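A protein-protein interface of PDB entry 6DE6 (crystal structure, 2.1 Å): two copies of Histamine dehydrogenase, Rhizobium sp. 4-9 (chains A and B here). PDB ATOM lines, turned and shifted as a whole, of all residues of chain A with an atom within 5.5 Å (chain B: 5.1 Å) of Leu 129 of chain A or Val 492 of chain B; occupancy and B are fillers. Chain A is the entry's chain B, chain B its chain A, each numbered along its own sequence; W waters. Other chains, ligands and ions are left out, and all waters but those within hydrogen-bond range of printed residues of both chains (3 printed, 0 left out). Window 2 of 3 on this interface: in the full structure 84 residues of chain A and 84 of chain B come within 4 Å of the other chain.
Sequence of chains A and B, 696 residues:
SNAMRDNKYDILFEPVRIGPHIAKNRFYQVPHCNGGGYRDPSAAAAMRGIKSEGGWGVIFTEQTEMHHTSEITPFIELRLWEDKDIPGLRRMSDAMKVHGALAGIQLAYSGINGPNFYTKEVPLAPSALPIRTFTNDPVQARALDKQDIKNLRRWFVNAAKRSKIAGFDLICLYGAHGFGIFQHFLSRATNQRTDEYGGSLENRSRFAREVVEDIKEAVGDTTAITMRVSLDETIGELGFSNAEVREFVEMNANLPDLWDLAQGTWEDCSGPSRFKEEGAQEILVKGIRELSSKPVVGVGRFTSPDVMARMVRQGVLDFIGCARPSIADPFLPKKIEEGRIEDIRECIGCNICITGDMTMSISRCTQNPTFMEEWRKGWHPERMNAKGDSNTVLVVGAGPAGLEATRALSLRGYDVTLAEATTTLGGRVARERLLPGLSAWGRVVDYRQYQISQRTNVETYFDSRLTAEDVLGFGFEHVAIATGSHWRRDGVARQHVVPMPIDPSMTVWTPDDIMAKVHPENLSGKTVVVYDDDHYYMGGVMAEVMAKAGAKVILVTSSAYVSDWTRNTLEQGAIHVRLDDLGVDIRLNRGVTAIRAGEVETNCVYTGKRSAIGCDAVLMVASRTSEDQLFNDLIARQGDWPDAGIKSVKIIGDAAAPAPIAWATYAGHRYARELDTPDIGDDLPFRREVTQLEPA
O of Val 497 of chain B is in hydrogen-bond range of NE2 of Gln 192 of chain A (2.8 Å).
The backbone NH (N) of Arg 488 of chain B lies within hydrogen-bond range of the backbone carbonyl oxygen (O) of Ser 623 of chain B (2.8 Å). The side-chain carboxylate of Asp 490 of chain B sits at hydrogen-bond distance from the backbone NH of Val 492 of chain B. The side-chain hydroxyl of Ser 623 of chain B lies within hydrogen-bond range of the backbone carbonyl oxygen of Val 492 of chain B (2.7 Å). N of Gln 192 of chain A sits at hydrogen-bond distance from OG of Ser 127 of chain A (2.9 Å). The backbone carbonyl oxygen (O) of Leu 129 of chain A sits at hydrogen-bond distance from the backbone NH (N) of Ala 141 of chain A, 2.9 Å away. NE2 of Gln 192 of chain A is in hydrogen-bond range of O of Ala 189 of chain A, 3.0 Å away.
Leu 129 of chain A touches Val 492 of chain B. Val 497 of chain B touches Leu 129 of chain A. CD of Pro 130 of chain A touches O of Ala 493 of chain B (3.3 Å). Pro 130 of chain A touches Arg 494 of chain B (CB to CZ, 3.8 Å). CG of Pro 130 of chain A touches CB of Ser 623 of chain B, at 3.6 Å. Ser 623 of chain B touches Gln 140 of chain A. O of Ala 189 of chain A touches CG2 of Val 497 of chain B, at 3.5 Å. Gln 192 of chain A touches Val 498 of chain B (NE2 to CG1, 3.6 Å).
Of chain B, only Val 492 and Val 497 come within 4 Å of Leu 129 of chain A. Printed residues of chain B within 4 Å of Ala 189 of chain A: Val 497 (3.5 Å). Of the printed residues of chain B, Gln 192 of chain A touches Val 497 and Val 498. Arg 488 of chain B touches none of the printed residues of chain A. Of the printed residues of chain A, Val 492 of chain B touches Leu 129 (3.7 Å). Printed residues of chain A within 4 Å of Arg 494 of chain B: Pro 130. Printed residues of chain A within 4 Å of Val 497 of chain B: Leu 129 (3.96 Å), Ala 189 (3.5 Å) and Gln 192 (2.8 Å).
Hydrophobic or aromatic side chains of chain B that line the printed part of chain A: Val 492, Val 497 and Val 498. Of the 12 printed residues of chain A, 5 touch a printed residue of chain B. Printed residues of chain A that touch a printed residue of chain B: Leu 129, Pro 130, Gln 140, Ala 189 and Gln 192. Among the printed residues, 9 pairs touch across the chains. Among the printed residues, no Asp or Glu carboxylate lies within 4 Å of a Lys or Arg side-chain nitrogen of the other chain.
No position is printed for both chains. Of the 9 pairs that touch across the chains among the printed residues, none has its exchanged pair printed and touching as well.
Water W3 bridges the backbone carbonyl oxygen (O) of Val 497 of chain B and the side-chain amide oxygen (OE1) of Gln 192 of chain A. Water W1 bridges the backbone carbonyl oxygen of Ile 131 of chain A and the guanidinium group of Arg 494 of chain B. Water W2 bridges the backbone carbonyl oxygen (O) of Ala 493 of chain B and the backbone carbonyl oxygen (O) of Pro 130 of chain A.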
ATOM      1  N   ILE A 112     -25.377 -18.098 -20.218  1.00  0.00           N
ATOM      2  CA  ILE A 112     -25.140 -19.304 -21.006  1.00  0.00           C
ATOM      3  C   ILE A 112     -23.641 -19.538 -21.263  1.00  0.00           C
ATOM      4  O   ILE A 112     -23.253 -20.550 -21.862  1.00  0.00           O
ATOM      5  CB  ILE A 112     -25.972 -19.247 -22.308  1.00  0.00           C
ATOM      6  CG1 ILE A 112     -26.293 -20.668 -22.764  1.00  0.00           C
ATOM      7  CG2 ILE A 112     -25.283 -18.449 -23.430  1.00  0.00           C
ATOM      8  CD1 ILE A 112     -27.239 -20.727 -23.899  1.00  0.00           C
ATOM      9  N   SER A 127     -33.015 -18.924 -22.876  1.00  0.00           N
ATOM     10  CA  SER A 127     -33.592 -20.124 -23.462  1.00  0.00           C
ATOM     11  C   SER A 127     -32.686 -21.310 -23.160  1.00  0.00           C
ATOM     12  O   SER A 127     -31.483 -21.150 -22.934  1.00  0.00           O
ATOM     13  CB  SER A 127     -33.791 -19.992 -24.994  1.00  0.00           C
ATOM     14  OG  SER A 127     -34.649 -18.903 -25.329  1.00  0.00           O
ATOM     15  N   ALA A 128     -33.286 -22.501 -23.126  1.00  0.00           N
ATOM     16  CA  ALA A 128     -32.595 -23.716 -22.701  1.00  0.00           C
ATOM     17  C   ALA A 128     -31.742 -24.254 -23.849  1.00  0.00           C
ATOM     18  O   ALA A 128     -32.269 -24.763 -24.840  1.00  0.00           O
ATOM     19  CB  ALA A 128     -33.617 -24.752 -22.227  1.00  0.00           C
ATOM     20  N   LEU A 129     -30.425 -24.161 -23.707  1.00  0.00           N
ATOM     21  CA  LEU A 129     -29.473 -24.610 -24.713  1.00  0.00           C
ATOM     22  C   LEU A 129     -28.211 -25.128 -24.028  1.00  0.00           C
ATOM     23  O   LEU A 129     -27.960 -24.821 -22.854  1.00  0.00           O
ATOM     24  CB  LEU A 129     -29.100 -23.472 -25.676  1.00  0.00           C
ATOM     25  CG  LEU A 129     -30.118 -22.977 -26.700  1.00  0.00           C
ATOM     26  CD1 LEU A 129     -29.591 -21.739 -27.413  1.00  0.00           C
ATOM     27  CD2 LEU A 129     -30.424 -24.043 -27.715  1.00  0.00           C
ATOM     28  N   PRO A 130     -27.375 -25.881 -24.748  1.00  0.00           N
ATOM     29  CA  PRO A 130     -26.026 -26.163 -24.243  1.00  0.00           C
ATOM     30  C   PRO A 130     -25.266 -24.885 -23.884  1.00  0.00           C
ATOM     31  O   PRO A 130     -25.379 -23.853 -24.554  1.00  0.00           O
ATOM     32  CB  PRO A 130     -25.361 -26.908 -25.410  1.00  0.00           C
ATOM     33  CG  PRO A 130     -26.482 -27.556 -26.128  1.00  0.00           C
ATOM     34  CD  PRO A 130     -27.637 -26.578 -26.024  1.00  0.00           C
ATOM     35  N   ILE A 131     -24.470 -24.975 -22.814  1.00  0.00           N
ATOM     36  CA  ILE A 131     -23.551 -23.906 -22.457  1.00  0.00           C
ATOM     37  C   ILE A 131     -22.629 -23.637 -23.639  1.00  0.00           C
ATOM     38  O   ILE A 131     -22.322 -24.533 -24.437  1.00  0.00           O
ATOM     39  CB  ILE A 131     -22.743 -24.275 -21.197  1.00  0.00           C
ATOM     40  CG1 ILE A 131     -23.579 -24.073 -19.926  1.00  0.00           C
ATOM     41  CG2 ILE A 131     -21.524 -23.443 -21.018  1.00  0.00           C
ATOM     42  CD1 ILE A 131     -23.823 -22.618 -19.550  1.00  0.00           C
ATOM     43  N   VAL A 139     -22.778 -29.390 -20.384  1.00  0.00           N
ATOM     44  CA  VAL A 139     -23.929 -29.010 -19.584  1.00  0.00           C
ATOM     45  C   VAL A 139     -24.760 -28.001 -20.349  1.00  0.00           C
ATOM     46  O   VAL A 139     -24.278 -27.298 -21.244  1.00  0.00           O
ATOM     47  CB  VAL A 139     -23.554 -28.437 -18.201  1.00  0.00           C
ATOM     48  CG1 VAL A 139     -22.602 -29.365 -17.460  1.00  0.00           C
ATOM     49  CG2 VAL A 139     -22.986 -27.066 -18.324  1.00  0.00           C
ATOM     50  N   GLN A 140     -26.026 -27.930 -19.966  1.00  0.00           N
ATOM     51  CA  GLN A 140     -26.972 -27.008 -20.573  1.00  0.00           C
ATOM     52  C   GLN A 140     -27.499 -26.059 -19.515  1.00  0.00           C
ATOM     53  O   GLN A 140     -27.397 -26.313 -18.312  1.00  0.00           O
ATOM     54  CB  GLN A 140     -28.140 -27.763 -21.240  1.00  0.00           C
ATOM     55  CG  GLN A 140     -27.705 -28.894 -22.166  1.00  0.00           C
ATOM     56  CD  GLN A 140     -28.829 -29.450 -23.056  1.00  0.00           C
ATOM     57  OE1 GLN A 140     -28.616 -30.401 -23.809  1.00  0.00           O
ATOM     58  NE2 GLN A 140     -30.001 -28.853 -22.986  1.00  0.00           N
ATOM     59  N   ALA A 141     -28.057 -24.951 -19.981  1.00  0.00           N
ATOM     60  CA  ALA A 141     -28.737 -23.989 -19.128  1.00  0.00           C
ATOM     61  C   ALA A 141     -30.237 -24.247 -19.117  1.00  0.00           C
ATOM     62  O   ALA A 141     -30.837 -24.593 -20.137  1.00  0.00           O
ATOM     63  CB  ALA A 141     -28.500 -22.551 -19.595  1.00  0.00           C
ATOM     64  N   ALA A 189     -30.262 -15.356 -31.303  1.00  0.00           N
ATOM     65  CA  ALA A 189     -29.764 -16.727 -31.285  1.00  0.00           C
ATOM     66  C   ALA A 189     -29.970 -17.364 -29.921  1.00  0.00           C
ATOM     67  O   ALA A 189     -30.400 -18.517 -29.820  1.00  0.00           O
ATOM     68  CB  ALA A 189     -28.279 -16.759 -31.656  1.00  0.00           C
ATOM     69  N   THR A 190     -29.612 -16.648 -28.859  1.00  0.00           N
ATOM     70  CA  THR A 190     -29.721 -17.195 -27.519  1.00  0.00           C
ATOM     71  C   THR A 190     -31.072 -16.911 -26.863  1.00  0.00           C
ATOM     72  O   THR A 190     -31.465 -17.650 -25.947  1.00  0.00           O
ATOM     73  CB  THR A 190     -28.599 -16.632 -26.645  1.00  0.00           C
ATOM     74  OG1 THR A 190     -28.483 -15.231 -26.890  1.00  0.00           O
ATOM     75  CG2 THR A 190     -27.266 -17.312 -26.936  1.00  0.00           C
ATOM     76  N   GLN A 192     -34.728 -17.049 -27.532  1.00  0.00           N
ATOM     77  CA  GLN A 192     -35.831 -17.524 -28.360  1.00  0.00           C
ATOM     78  C   GLN A 192     -37.157 -17.481 -27.609  1.00  0.00           C
ATOM     79  O   GLN A 192     -38.120 -18.146 -28.007  1.00  0.00           O
ATOM     80  CB  GLN A 192     -35.522 -18.939 -28.854  1.00  0.00           C
ATOM     81  CG  GLN A 192     -34.324 -18.982 -29.820  1.00  0.00           C
ATOM     82  CD  GLN A 192     -33.873 -20.381 -30.164  1.00  0.00           C
ATOM     83  OE1 GLN A 192     -34.684 -21.310 -30.251  1.00  0.00           O
ATOM     84  NE2 GLN A 192     -32.566 -20.547 -30.358  1.00  0.00           N
ATOM     85  N   ARG B 488     -32.328 -34.621 -29.234  1.00  0.00           N
ATOM     86  CA  ARG B 488     -33.056 -33.800 -30.191  1.00  0.00           C
ATOM     87  C   ARG B 488     -32.872 -34.295 -31.617  1.00  0.00           C
ATOM     88  O   ARG B 488     -31.812 -34.793 -32.000  1.00  0.00           O
ATOM     89  CB  ARG B 488     -32.600 -32.348 -30.080  1.00  0.00           C
ATOM     90  CG  ARG B 488     -32.887 -31.752 -28.717  1.00  0.00           C
ATOM     91  CD  ARG B 488     -32.526 -30.261 -28.642  1.00  0.00           C
ATOM     92  NE  ARG B 488     -33.300 -29.473 -29.592  1.00  0.00           N
ATOM     93  CZ  ARG B 488     -33.570 -28.182 -29.450  1.00  0.00           C
ATOM     94  NH1 ARG B 488     -33.127 -27.525 -28.388  1.00  0.00           N
ATOM     95  NH2 ARG B 488     -34.275 -27.546 -30.384  1.00  0.00           N
ATOM     96  N   ASP B 490     -33.665 -32.149 -34.313  1.00  0.00           N
ATOM     97  CA  ASP B 490     -33.587 -30.981 -35.185  1.00  0.00           C
ATOM     98  C   ASP B 490     -32.177 -30.420 -35.346  1.00  0.00           C
ATOM     99  O   ASP B 490     -32.016 -29.373 -35.978  1.00  0.00           O
ATOM    100  CB  ASP B 490     -34.534 -29.889 -34.665  1.00  0.00           C
ATOM    101  CG  ASP B 490     -34.267 -29.520 -33.214  1.00  0.00           C
ATOM    102  OD1 ASP B 490     -33.217 -29.926 -32.659  1.00  0.00           O
ATOM    103  OD2 ASP B 490     -35.123 -28.836 -32.625  1.00  0.00           O
ATOM    104  N   GLY B 491     -31.153 -31.097 -34.821  1.00  0.00           N
ATOM    105  CA  GLY B 491     -29.782 -30.704 -35.016  1.00  0.00           C
ATOM    106  C   GLY B 491     -29.283 -29.596 -34.111  1.00  0.00           C
ATOM    107  O   GLY B 491     -28.124 -29.181 -34.252  1.00  0.00           O
ATOM    108  N   VAL B 492     -30.105 -29.119 -33.183  1.00  0.00           N
ATOM    109  CA  VAL B 492     -29.758 -27.989 -32.332  1.00  0.00           C
ATOM    110  C   VAL B 492     -28.862 -28.457 -31.191  1.00  0.00           C
ATOM    111  O   VAL B 492     -29.154 -29.450 -30.519  1.00  0.00           O
ATOM    112  CB  VAL B 492     -31.030 -27.317 -31.792  1.00  0.00           C
ATOM    113  CG1 VAL B 492     -30.699 -26.311 -30.685  1.00  0.00           C
ATOM    114  CG2 VAL B 492     -31.804 -26.644 -32.930  1.00  0.00           C
ATOM    115  N   ALA B 493     -27.762 -27.740 -30.979  1.00  0.00           N
ATOM    116  CA  ALA B 493     -26.878 -27.953 -29.842  1.00  0.00           C
ATOM    117  C   ALA B 493     -25.973 -26.738 -29.652  1.00  0.00           C
ATOM    118  O   ALA B 493     -26.315 -25.822 -28.900  1.00  0.00           O
ATOM    119  CB  ALA B 493     -26.054 -29.228 -30.037  1.00  0.00           C
ATOM    120  N   ARG B 494     -24.826 -26.723 -30.338  1.00  0.00           N
ATOM    121  CA  ARG B 494     -23.862 -25.626 -30.289  1.00  0.00           C
ATOM    122  C   ARG B 494     -23.704 -24.949 -31.649  1.00  0.00           C
ATOM    123  O   ARG B 494     -23.867 -23.729 -31.748  1.00  0.00           O
ATOM    124  CB  ARG B 494     -22.509 -26.171 -29.792  1.00  0.00           C
ATOM    125  CG  ARG B 494     -22.558 -26.705 -28.384  1.00  0.00           C
ATOM    126  CD  ARG B 494     -21.516 -27.803 -28.134  1.00  0.00           C
ATOM    127  NE  ARG B 494     -21.592 -28.199 -26.732  1.00  0.00           N
ATOM    128  CZ  ARG B 494     -22.424 -29.107 -26.227  1.00  0.00           C
ATOM    129  NH1 ARG B 494     -23.268 -29.790 -27.001  1.00  0.00           N
ATOM    130  NH2 ARG B 494     -22.420 -29.318 -24.911  1.00  0.00           N
ATOM    131  N   HIS B 496     -25.689 -25.144 -34.292  1.00  0.00           N
ATOM    132  CA  HIS B 496     -27.005 -24.610 -34.626  1.00  0.00           C
ATOM    133  C   HIS B 496     -27.774 -24.335 -33.335  1.00  0.00           C
ATOM    134  O   HIS B 496     -27.863 -25.208 -32.459  1.00  0.00           O
ATOM    135  CB  HIS B 496     -27.821 -25.609 -35.479  1.00  0.00           C
ATOM    136  CG  HIS B 496     -27.116 -26.111 -36.699  1.00  0.00           C
ATOM    137  ND1 HIS B 496     -27.228 -25.500 -37.932  1.00  0.00           N
ATOM    138  CD2 HIS B 496     -26.289 -27.168 -36.877  1.00  0.00           C
ATOM    139  CE1 HIS B 496     -26.497 -26.160 -38.812  1.00  0.00           C
ATOM    140  NE2 HIS B 496     -25.920 -27.179 -38.199  1.00  0.00           N
ATOM    141  N   VAL B 497     -28.370 -23.155 -33.221  1.00  0.00           N
ATOM    142  CA  VAL B 497     -29.253 -22.875 -32.092  1.00  0.00           C
ATOM    143  C   VAL B 497     -30.702 -22.870 -32.501  1.00  0.00           C
ATOM    144  O   VAL B 497     -31.576 -22.846 -31.622  1.00  0.00           O
ATOM    145  CB  VAL B 497     -28.885 -21.552 -31.384  1.00  0.00           C
ATOM    146  CG1 VAL B 497     -27.478 -21.654 -30.763  1.00  0.00           C
ATOM    147  CG2 VAL B 497     -28.962 -20.410 -32.350  1.00  0.00           C
ATOM    148  N   VAL B 498     -30.984 -22.925 -33.800  1.00  0.00           N
ATOM    149  CA  VAL B 498     -32.318 -23.198 -34.325  1.00  0.00           C
ATOM    150  C   VAL B 498     -32.206 -24.325 -35.347  1.00  0.00           C
ATOM    151  O   VAL B 498     -31.118 -24.617 -35.870  1.00  0.00           O
ATOM    152  CB  VAL B 498     -32.946 -21.936 -34.951  1.00  0.00           C
ATOM    153  CG1 VAL B 498     -32.960 -20.803 -33.922  1.00  0.00           C
ATOM    154  CG2 VAL B 498     -32.185 -21.550 -36.191  1.00  0.00           C
ATOM    155  N   PRO B 499     -33.314 -25.001 -35.626  1.00  0.00           N
ATOM    156  CA  PRO B 499     -33.256 -26.237 -36.416  1.00  0.00           C
ATOM    157  C   PRO B 499     -32.531 -26.056 -37.736  1.00  0.00           C
ATOM    158  O   PRO B 499     -32.680 -25.041 -38.421  1.00  0.00           O
ATOM    159  CB  PRO B 499     -34.731 -26.582 -36.621  1.00  0.00           C
ATOM    160  CG  PRO B 499     -35.388 -26.061 -35.386  1.00  0.00           C
ATOM    161  CD  PRO B 499     -34.656 -24.775 -35.065  1.00  0.00           C
ATOM    162  N   ALA B 622     -26.734 -34.504 -31.052  1.00  0.00           N
ATOM    163  CA  ALA B 622     -26.742 -33.053 -30.921  1.00  0.00           C
ATOM    164  C   ALA B 622     -26.776 -32.674 -29.449  1.00  0.00           C
ATOM    165  O   ALA B 622     -25.738 -32.646 -28.771  1.00  0.00           O
ATOM    166  CB  ALA B 622     -27.945 -32.468 -31.674  1.00  0.00           C
ATOM    167  N   SER B 623     -27.968 -32.410 -28.940  1.00  0.00           N
ATOM    168  CA  SER B 623     -28.150 -32.102 -27.532  1.00  0.00           C
ATOM    169  C   SER B 623     -29.527 -32.606 -27.116  1.00  0.00           C
ATOM    170  O   SER B 623     -30.252 -33.237 -27.901  1.00  0.00           O
ATOM    171  CB  SER B 623     -27.978 -30.594 -27.271  1.00  0.00           C
ATOM    172  OG  SER B 623     -29.032 -29.825 -27.831  1.00  0.00           O
HETATM  173  O   HOH W   1     -20.668 -26.667 -24.619  1.00  0.00           O
HETATM  174  O   HOH W   2     -25.419 -23.613 -27.469  1.00  0.00           O
HETATM  175  O   HOH W   3     -33.797 -23.885 -30.629  1.00  0.00           O
